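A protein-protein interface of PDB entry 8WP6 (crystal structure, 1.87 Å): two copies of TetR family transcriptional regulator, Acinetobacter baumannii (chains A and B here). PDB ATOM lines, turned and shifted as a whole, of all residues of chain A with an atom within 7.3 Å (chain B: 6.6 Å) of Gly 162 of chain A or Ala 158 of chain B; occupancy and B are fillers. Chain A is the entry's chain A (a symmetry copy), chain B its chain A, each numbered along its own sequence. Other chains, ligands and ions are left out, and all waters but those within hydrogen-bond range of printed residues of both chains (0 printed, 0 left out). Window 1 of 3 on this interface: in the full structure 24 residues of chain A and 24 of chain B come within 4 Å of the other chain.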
ATOM      1  N   LEU A 156     -32.627   5.014   1.317  1.00  0.00           N
ATOM      2  CA  LEU A 156     -31.419   4.364   0.814  1.00  0.00           C
ATOM      3  C   LEU A 156     -30.255   4.534   1.784  1.00  0.00           C
ATOM      4  O   LEU A 156     -29.516   3.581   2.054  1.00  0.00           O
ATOM      5  CB  LEU A 156     -31.063   4.932  -0.563  1.00  0.00           C
ATOM      6  CG  LEU A 156     -31.960   4.554  -1.749  1.00  0.00           C
ATOM      7  CD1 LEU A 156     -31.498   5.233  -3.037  1.00  0.00           C
ATOM      8  CD2 LEU A 156     -32.020   3.043  -1.962  1.00  0.00           C
ATOM      9  N   ILE A 157     -30.072   5.746   2.319  1.00  0.00           N
ATOM     10  CA  ILE A 157     -29.019   5.959   3.308  1.00  0.00           C
ATOM     11  C   ILE A 157     -29.291   5.125   4.552  1.00  0.00           C
ATOM     12  O   ILE A 157     -28.390   4.473   5.093  1.00  0.00           O
ATOM     13  CB  ILE A 157     -28.894   7.458   3.636  1.00  0.00           C
ATOM     14  CG1 ILE A 157     -28.196   8.187   2.488  1.00  0.00           C
ATOM     15  CG2 ILE A 157     -28.149   7.667   4.970  1.00  0.00           C
ATOM     16  CD1 ILE A 157     -28.102   9.679   2.687  1.00  0.00           C
ATOM     17  N   ALA A 158     -30.542   5.110   5.009  1.00  0.00           N
ATOM     18  CA  ALA A 158     -30.889   4.328   6.188  1.00  0.00           C
ATOM     19  C   ALA A 158     -30.567   2.858   5.979  1.00  0.00           C
ATOM     20  O   ALA A 158     -30.048   2.195   6.884  1.00  0.00           O
ATOM     21  CB  ALA A 158     -32.369   4.507   6.524  1.00  0.00           C
ATOM     22  N   PHE A 159     -30.843   2.343   4.780  1.00  0.00           N
ATOM     23  CA  PHE A 159     -30.609   0.931   4.505  1.00  0.00           C
ATOM     24  C   PHE A 159     -29.129   0.586   4.581  1.00  0.00           C
ATOM     25  O   PHE A 159     -28.741  -0.383   5.243  1.00  0.00           O
ATOM     26  CB  PHE A 159     -31.160   0.546   3.134  1.00  0.00           C
ATOM     27  CG  PHE A 159     -30.941  -0.892   2.809  1.00  0.00           C
ATOM     28  CD1 PHE A 159     -31.700  -1.871   3.434  1.00  0.00           C
ATOM     29  CD2 PHE A 159     -29.945  -1.278   1.936  1.00  0.00           C
ATOM     30  CE1 PHE A 159     -31.483  -3.211   3.168  1.00  0.00           C
ATOM     31  CE2 PHE A 159     -29.725  -2.618   1.662  1.00  0.00           C
ATOM     32  CZ  PHE A 159     -30.494  -3.584   2.280  1.00  0.00           C
ATOM     33  N   VAL A 160     -28.285   1.349   3.883  1.00  0.00           N
ATOM     34  CA  VAL A 160     -26.876   0.982   3.834  1.00  0.00           C
ATOM     35  C   VAL A 160     -26.217   1.199   5.194  1.00  0.00           C
ATOM     36  O   VAL A 160     -25.363   0.411   5.607  1.00  0.00           O
ATOM     37  CB  VAL A 160     -26.141   1.726   2.699  1.00  0.00           C
ATOM     38  CG1 VAL A 160     -26.762   1.390   1.337  1.00  0.00           C
ATOM     39  CG2 VAL A 160     -26.164   3.223   2.923  1.00  0.00           C
ATOM     40  N   CYS A 161     -26.611   2.246   5.924  1.00  0.00           N
ATOM     41  CA  CYS A 161     -26.063   2.428   7.267  1.00  0.00           C
ATOM     42  C   CYS A 161     -26.527   1.315   8.195  1.00  0.00           C
ATOM     43  O   CYS A 161     -25.745   0.819   9.015  1.00  0.00           O
ATOM     44  CB  CYS A 161     -26.462   3.790   7.831  1.00  0.00           C
ATOM     45  SG  CYS A 161     -25.779   5.191   6.934  1.00  0.00           S
ATOM     46  N   GLY A 162     -27.789   0.906   8.069  1.00  0.00           N
ATOM     47  CA  GLY A 162     -28.297  -0.177   8.897  1.00  0.00           C
ATOM     48  C   GLY A 162     -27.650  -1.507   8.574  1.00  0.00           C
ATOM     49  O   GLY A 162     -27.309  -2.277   9.477  1.00  0.00           O
ATOM     50  N   LEU A 163     -27.462  -1.790   7.285  1.00  0.00           N
ATOM     51  CA  LEU A 163     -26.813  -3.034   6.888  1.00  0.00           C
ATOM     52  C   LEU A 163     -25.382  -3.090   7.405  1.00  0.00           C
ATOM     53  O   LEU A 163     -24.944  -4.111   7.949  1.00  0.00           O
ATOM     54  CB  LEU A 163     -26.857  -3.175   5.366  1.00  0.00           C
ATOM     55  CG  LEU A 163     -26.589  -4.576   4.822  1.00  0.00           C
ATOM     56  CD1 LEU A 163     -27.357  -5.626   5.612  1.00  0.00           C
ATOM     57  CD2 LEU A 163     -26.930  -4.631   3.342  1.00  0.00           C
ATOM     58  N   GLU A 164     -24.638  -1.992   7.258  1.00  0.00           N
ATOM     59  CA  GLU A 164     -23.272  -1.964   7.778  1.00  0.00           C
ATOM     60  C   GLU A 164     -23.250  -2.015   9.303  1.00  0.00           C
ATOM     61  O   GLU A 164     -22.324  -2.586   9.888  1.00  0.00           O
ATOM     62  CB  GLU A 164     -22.547  -0.728   7.245  1.00  0.00           C
ATOM     63  CG  GLU A 164     -22.435  -0.740   5.716  1.00  0.00           C
ATOM     64  CD  GLU A 164     -21.884   0.550   5.137  1.00  0.00           C
ATOM     65  OE1 GLU A 164     -22.346   1.637   5.550  1.00  0.00           O
ATOM     66  OE2 GLU A 164     -20.999   0.475   4.255  1.00  0.00           O
ATOM     67  N   GLY A 165     -24.264  -1.454   9.963  1.00  0.00           N
ATOM     68  CA  GLY A 165     -24.354  -1.593  11.407  1.00  0.00           C
ATOM     69  C   GLY A 165     -24.545  -3.032  11.842  1.00  0.00           C
ATOM     70  O   GLY A 165     -23.975  -3.469  12.846  1.00  0.00           O
ATOM     71  N   ILE A 166     -25.332  -3.798  11.084  1.00  0.00           N
ATOM     72  CA  ILE A 166     -25.586  -5.187  11.449  1.00  0.00           C
ATOM     73  C   ILE A 166     -24.353  -6.042  11.175  1.00  0.00           C
ATOM     74  O   ILE A 166     -24.070  -7.005  11.902  1.00  0.00           O
ATOM     75  CB  ILE A 166     -26.828  -5.713  10.703  1.00  0.00           C
ATOM     76  CG1 ILE A 166     -28.095  -5.000  11.178  1.00  0.00           C
ATOM     77  CG2 ILE A 166     -27.030  -7.172  10.995  1.00  0.00           C
ATOM     78  CD1 ILE A 166     -28.081  -4.624  12.635  1.00  0.00           C
ATOM     79  N   TYR A 167     -23.594  -5.705  10.124  1.00  0.00           N
ATOM     80  CA  TYR A 167     -22.321  -6.383   9.874  1.00  0.00           C
ATOM     81  C   TYR A 167     -21.364  -6.243  11.052  1.00  0.00           C
ATOM     82  O   TYR A 167     -20.586  -7.162  11.340  1.00  0.00           O
ATOM     83  CB  TYR A 167     -21.662  -5.828   8.613  1.00  0.00           C
ATOM     84  CG  TYR A 167     -22.364  -6.202   7.338  1.00  0.00           C
ATOM     85  CD1 TYR A 167     -23.169  -7.331   7.271  1.00  0.00           C
ATOM     86  CD2 TYR A 167     -22.232  -5.420   6.200  1.00  0.00           C
ATOM     87  CE1 TYR A 167     -23.817  -7.677   6.101  1.00  0.00           C
ATOM     88  CE2 TYR A 167     -22.883  -5.756   5.025  1.00  0.00           C
ATOM     89  CZ  TYR A 167     -23.668  -6.882   4.982  1.00  0.00           C
ATOM     90  OH  TYR A 167     -24.312  -7.215   3.810  1.00  0.00           O
ATOM     91  N   LYS A 168     -21.378  -5.088  11.722  1.00  0.00           N
ATOM     92  CA  LYS A 168     -20.467  -4.871  12.841  1.00  0.00           C
ATOM     93  C   LYS A 168     -20.753  -5.798  14.011  1.00  0.00           C
ATOM     94  O   LYS A 168     -19.899  -5.942  14.890  1.00  0.00           O
ATOM     95  CB  LYS A 168     -20.533  -3.421  13.324  1.00  0.00           C
ATOM     96  CG  LYS A 168     -19.898  -2.403  12.389  1.00  0.00           C
ATOM     97  CD  LYS A 168     -19.785  -1.042  13.074  1.00  0.00           C
ATOM     98  CE  LYS A 168     -20.632   0.007  12.376  1.00  0.00           C
ATOM     99  NZ  LYS A 168     -19.890   0.663  11.260  1.00  0.00           N
ATOM    100  N   PHE A 179     -23.470  -7.454   0.468  1.00  0.00           N
ATOM    101  CA  PHE A 179     -23.886  -6.056   0.570  1.00  0.00           C
ATOM    102  C   PHE A 179     -24.338  -5.491  -0.772  1.00  0.00           C
ATOM    103  O   PHE A 179     -25.378  -4.830  -0.856  1.00  0.00           O
ATOM    104  CB  PHE A 179     -22.755  -5.208   1.151  1.00  0.00           C
ATOM    105  CG  PHE A 179     -23.083  -3.741   1.235  1.00  0.00           C
ATOM    106  CD1 PHE A 179     -23.743  -3.223   2.335  1.00  0.00           C
ATOM    107  CD2 PHE A 179     -22.696  -2.875   0.222  1.00  0.00           C
ATOM    108  CE1 PHE A 179     -24.040  -1.872   2.410  1.00  0.00           C
ATOM    109  CE2 PHE A 179     -22.986  -1.525   0.293  1.00  0.00           C
ATOM    110  CZ  PHE A 179     -23.658  -1.022   1.390  1.00  0.00           C
ATOM    111  N   TRP B 126     -35.021 -12.371  16.575  1.00  0.00           N
ATOM    112  CA  TRP B 126     -35.822 -11.364  15.887  1.00  0.00           C
ATOM    113  C   TRP B 126     -35.902 -11.664  14.396  1.00  0.00           C
ATOM    114  O   TRP B 126     -36.982 -11.614  13.796  1.00  0.00           O
ATOM    115  CB  TRP B 126     -35.204  -9.989  16.127  1.00  0.00           C
ATOM    116  CG  TRP B 126     -36.001  -8.803  15.661  1.00  0.00           C
ATOM    117  CD1 TRP B 126     -37.343  -8.744  15.409  1.00  0.00           C
ATOM    118  CD2 TRP B 126     -35.478  -7.502  15.369  1.00  0.00           C
ATOM    119  NE1 TRP B 126     -37.689  -7.476  14.990  1.00  0.00           N
ATOM    120  CE2 TRP B 126     -36.559  -6.697  14.960  1.00  0.00           C
ATOM    121  CE3 TRP B 126     -34.197  -6.939  15.421  1.00  0.00           C
ATOM    122  CZ2 TRP B 126     -36.401  -5.359  14.605  1.00  0.00           C
ATOM    123  CZ3 TRP B 126     -34.040  -5.609  15.065  1.00  0.00           C
ATOM    124  CH2 TRP B 126     -35.139  -4.833  14.665  1.00  0.00           C
ATOM    125  N   ALA B 153     -35.954 -10.654   5.356  1.00  0.00           N
ATOM    126  CA  ALA B 153     -35.945 -10.389   6.791  1.00  0.00           C
ATOM    127  C   ALA B 153     -34.719  -9.590   7.211  1.00  0.00           C
ATOM    128  O   ALA B 153     -34.828  -8.653   8.011  1.00  0.00           O
ATOM    129  CB  ALA B 153     -36.014 -11.700   7.573  1.00  0.00           C
ATOM    130  N   TRP B 154     -33.534  -9.955   6.709  1.00  0.00           N
ATOM    131  CA  TRP B 154     -32.344  -9.183   7.062  1.00  0.00           C
ATOM    132  C   TRP B 154     -32.434  -7.763   6.519  1.00  0.00           C
ATOM    133  O   TRP B 154     -32.011  -6.810   7.186  1.00  0.00           O
ATOM    134  CB  TRP B 154     -31.068  -9.867   6.556  1.00  0.00           C
ATOM    135  CG  TRP B 154     -30.594 -11.026   7.410  1.00  0.00           C
ATOM    136  CD1 TRP B 154     -30.322 -12.296   6.984  1.00  0.00           C
ATOM    137  CD2 TRP B 154     -30.353 -11.020   8.827  1.00  0.00           C
ATOM    138  NE1 TRP B 154     -29.917 -13.075   8.044  1.00  0.00           N
ATOM    139  CE2 TRP B 154     -29.928 -12.318   9.184  1.00  0.00           C
ATOM    140  CE3 TRP B 154     -30.451 -10.046   9.826  1.00  0.00           C
ATOM    141  CZ2 TRP B 154     -29.607 -12.665  10.494  1.00  0.00           C
ATOM    142  CZ3 TRP B 154     -30.128 -10.394  11.129  1.00  0.00           C
ATOM    143  CH2 TRP B 154     -29.714 -11.693  11.449  1.00  0.00           C
ATOM    144  N   ARG B 155     -33.001  -7.594   5.324  1.00  0.00           N
ATOM    145  CA  ARG B 155     -33.108  -6.253   4.759  1.00  0.00           C
ATOM    146  C   ARG B 155     -34.082  -5.395   5.557  1.00  0.00           C
ATOM    147  O   ARG B 155     -33.833  -4.201   5.761  1.00  0.00           O
ATOM    148  CB  ARG B 155     -33.518  -6.337   3.286  1.00  0.00           C
ATOM    149  CG  ARG B 155     -32.388  -6.834   2.382  1.00  0.00           C
ATOM    150  CD  ARG B 155     -32.596  -6.437   0.921  1.00  0.00           C
ATOM    151  NE  ARG B 155     -33.717  -7.144   0.310  1.00  0.00           N
ATOM    152  CZ  ARG B 155     -33.594  -8.220  -0.458  1.00  0.00           C
ATOM    153  NH1 ARG B 155     -32.414  -8.771  -0.691  1.00  0.00           N
ATOM    154  NH2 ARG B 155     -34.681  -8.752  -1.012  1.00  0.00           N
ATOM    155  N   LEU B 156     -35.190  -5.988   6.017  1.00  0.00           N
ATOM    156  CA  LEU B 156     -36.144  -5.257   6.847  1.00  0.00           C
ATOM    157  C   LEU B 156     -35.524  -4.859   8.182  1.00  0.00           C
ATOM    158  O   LEU B 156     -35.696  -3.725   8.643  1.00  0.00           O
ATOM    159  CB  LEU B 156     -37.397  -6.111   7.067  1.00  0.00           C
ATOM    160  CG  LEU B 156     -38.341  -6.319   5.875  1.00  0.00           C
ATOM    161  CD1 LEU B 156     -39.514  -7.225   6.246  1.00  0.00           C
ATOM    162  CD2 LEU B 156     -38.870  -4.996   5.327  1.00  0.00           C
ATOM    163  N   ILE B 157     -34.796  -5.781   8.822  1.00  0.00           N
ATOM    164  CA  ILE B 157     -34.117  -5.441  10.069  1.00  0.00           C
ATOM    165  C   ILE B 157     -33.073  -4.362   9.822  1.00  0.00           C
ATOM    166  O   ILE B 157     -32.969  -3.389  10.580  1.00  0.00           O
ATOM    167  CB  ILE B 157     -33.500  -6.704  10.698  1.00  0.00           C
ATOM    168  CG1 ILE B 157     -34.598  -7.560  11.332  1.00  0.00           C
ATOM    169  CG2 ILE B 157     -32.416  -6.330  11.729  1.00  0.00           C
ATOM    170  CD1 ILE B 157     -34.095  -8.862  11.904  1.00  0.00           C
ATOM    171  N   ALA B 158     -32.303  -4.500   8.744  1.00  0.00           N
ATOM    172  CA  ALA B 158     -31.287  -3.505   8.429  1.00  0.00           C
ATOM    173  C   ALA B 158     -31.910  -2.130   8.250  1.00  0.00           C
ATOM    174  O   ALA B 158     -31.362  -1.128   8.722  1.00  0.00           O
ATOM    175  CB  ALA B 158     -30.522  -3.911   7.170  1.00  0.00           C
ATOM    176  N   PHE B 159     -33.070  -2.073   7.595  1.00  0.00           N
ATOM    177  CA  PHE B 159     -33.717  -0.792   7.337  1.00  0.00           C
ATOM    178  C   PHE B 159     -34.136  -0.110   8.630  1.00  0.00           C
ATOM    179  O   PHE B 159     -33.850   1.075   8.839  1.00  0.00           O
ATOM    180  CB  PHE B 159     -34.931  -0.970   6.429  1.00  0.00           C
ATOM    181  CG  PHE B 159     -35.625   0.317   6.139  1.00  0.00           C
ATOM    182  CD1 PHE B 159     -35.058   1.235   5.267  1.00  0.00           C
ATOM    183  CD2 PHE B 159     -36.806   0.643   6.775  1.00  0.00           C
ATOM    184  CE1 PHE B 159     -35.674   2.447   5.018  1.00  0.00           C
ATOM    185  CE2 PHE B 159     -37.431   1.855   6.526  1.00  0.00           C
ATOM    186  CZ  PHE B 159     -36.863   2.757   5.648  1.00  0.00           C
ATOM    187  N   VAL B 160     -34.846  -0.830   9.502  1.00  0.00           N
ATOM    188  CA  VAL B 160     -35.367  -0.179  10.696  1.00  0.00           C
ATOM    189  C   VAL B 160     -34.231   0.175  11.653  1.00  0.00           C
ATOM    190  O   VAL B 160     -34.265   1.225  12.301  1.00  0.00           O
ATOM    191  CB  VAL B 160     -36.458  -1.038  11.372  1.00  0.00           C
ATOM    192  CG1 VAL B 160     -37.634  -1.274  10.414  1.00  0.00           C
ATOM    193  CG2 VAL B 160     -35.899  -2.363  11.841  1.00  0.00           C
ATOM    194  N   CYS B 161     -33.201  -0.669  11.746  1.00  0.00           N
ATOM    195  CA  CYS B 161     -32.058  -0.312  12.586  1.00  0.00           C
ATOM    196  C   CYS B 161     -31.320   0.888  12.013  1.00  0.00           C
ATOM    197  O   CYS B 161     -30.886   1.772  12.762  1.00  0.00           O
ATOM    198  CB  CYS B 161     -31.108  -1.499  12.734  1.00  0.00           C
ATOM    199  SG  CYS B 161     -31.812  -2.906  13.604  1.00  0.00           S
ATOM    200  N   GLY B 162     -31.181   0.939  10.687  1.00  0.00           N
ATOM    201  CA  GLY B 162     -30.518   2.072  10.062  1.00  0.00           C
ATOM    202  C   GLY B 162     -31.304   3.357  10.204  1.00  0.00           C
ATOM    203  O   GLY B 162     -30.734   4.417  10.478  1.00  0.00           O
ATOM    204  N   LEU B 163     -32.624   3.280  10.031  1.00  0.00           N
ATOM    205  CA  LEU B 163     -33.460   4.464  10.186  1.00  0.00           C
ATOM    206  C   LEU B 163     -33.389   4.999  11.609  1.00  0.00           C
ATOM    207  O   LEU B 163     -33.238   6.208  11.826  1.00  0.00           O
ATOM    208  CB  LEU B 163     -34.901   4.132   9.792  1.00  0.00           C
ATOM    209  CG  LEU B 163     -35.805   5.330   9.515  1.00  0.00           C
ATOM    210  CD1 LEU B 163     -35.096   6.361   8.647  1.00  0.00           C
ATOM    211  CD2 LEU B 163     -37.103   4.863   8.877  1.00  0.00           C
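Printed residues of chain A that touch a printed residue of chain B: Ala 158, Phe 159, Gly 162 and Leu 163.
Hydrophobic or aromatic side chains of chain A that line the printed part of chain B: Ala 158, Phe 159 and Leu 163.
Along chain A the printed residues that touch a printed residue of chain B span positions 158 to 163.
Printed residues of chain B that touch a printed residue of chain A: Arg 155, Ala 158, Gly 162 and Leu 163.
Among the printed residues, 6 pairs touch across the chains.
Among the printed residues, no Asp or Glu carboxylate lies within 4 Å of a Lys or Arg side-chain nitrogen of the other chain.
Of the printed residues of chain B, Phe 159 of chain A touches Arg 155 (3.6 Å).
Of chain B, only Ala 158 and Gly 162 come within 4 Å of Gly 162 of chain A.
Ile 166 of chain A touches none of the printed residues of chain B.
Lys 168 of chain A touches none of the printed residues of chain B.
Of the printed residues of chain A, Arg 155 of chain B touches Phe 159.
Of the printed residues of chain A, Ala 158 of chain B touches Gly 162 (3.2 Å) and Leu 163 (3.7 Å).
Of the printed residues of chain A, Gly 162 of chain B touches Ala 158 and Gly 162.
Printed residues of chain A within 4 Å of Leu 163 of chain B: Ala 158.
The nearest residue of chain B that does not touch Gly 162 of chain A is Cys 161 of chain B (4.5 Å).
The nearest printed residue of chain A that does not touch Ala 158 of chain B is Ala 158 of chain A (4.02 Å).
Ala 158 of chain A touches Gly 162 of chain B, and with the chains exchanged Gly 162 of chain A touches Ala 158 of chain B.
Ala 158 of chain A touches Leu 163 of chain B, and with the chains exchanged Leu 163 of chain A touches Ala 158 of chain B.
Gly 162 of chain B touches its own counterpart, Gly 162 of chain A.
8 positions are printed for both chains.
Gly 162 of chain B touches Ala 158 of chain A (CA to O, 3.2 Å).
CB of Ala 158 of chain A touches N of Leu 163 of chain B (3.7 Å).
Phe 159 of chain A touches Arg 155 of chain B.
Gly 162 of chain A touches Ala 158 of chain B.
Gly 162 of chain A touches Gly 162 of chain B.
Ala 158 of chain B touches Leu 163 of chain A (CB to N, 3.7 Å).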
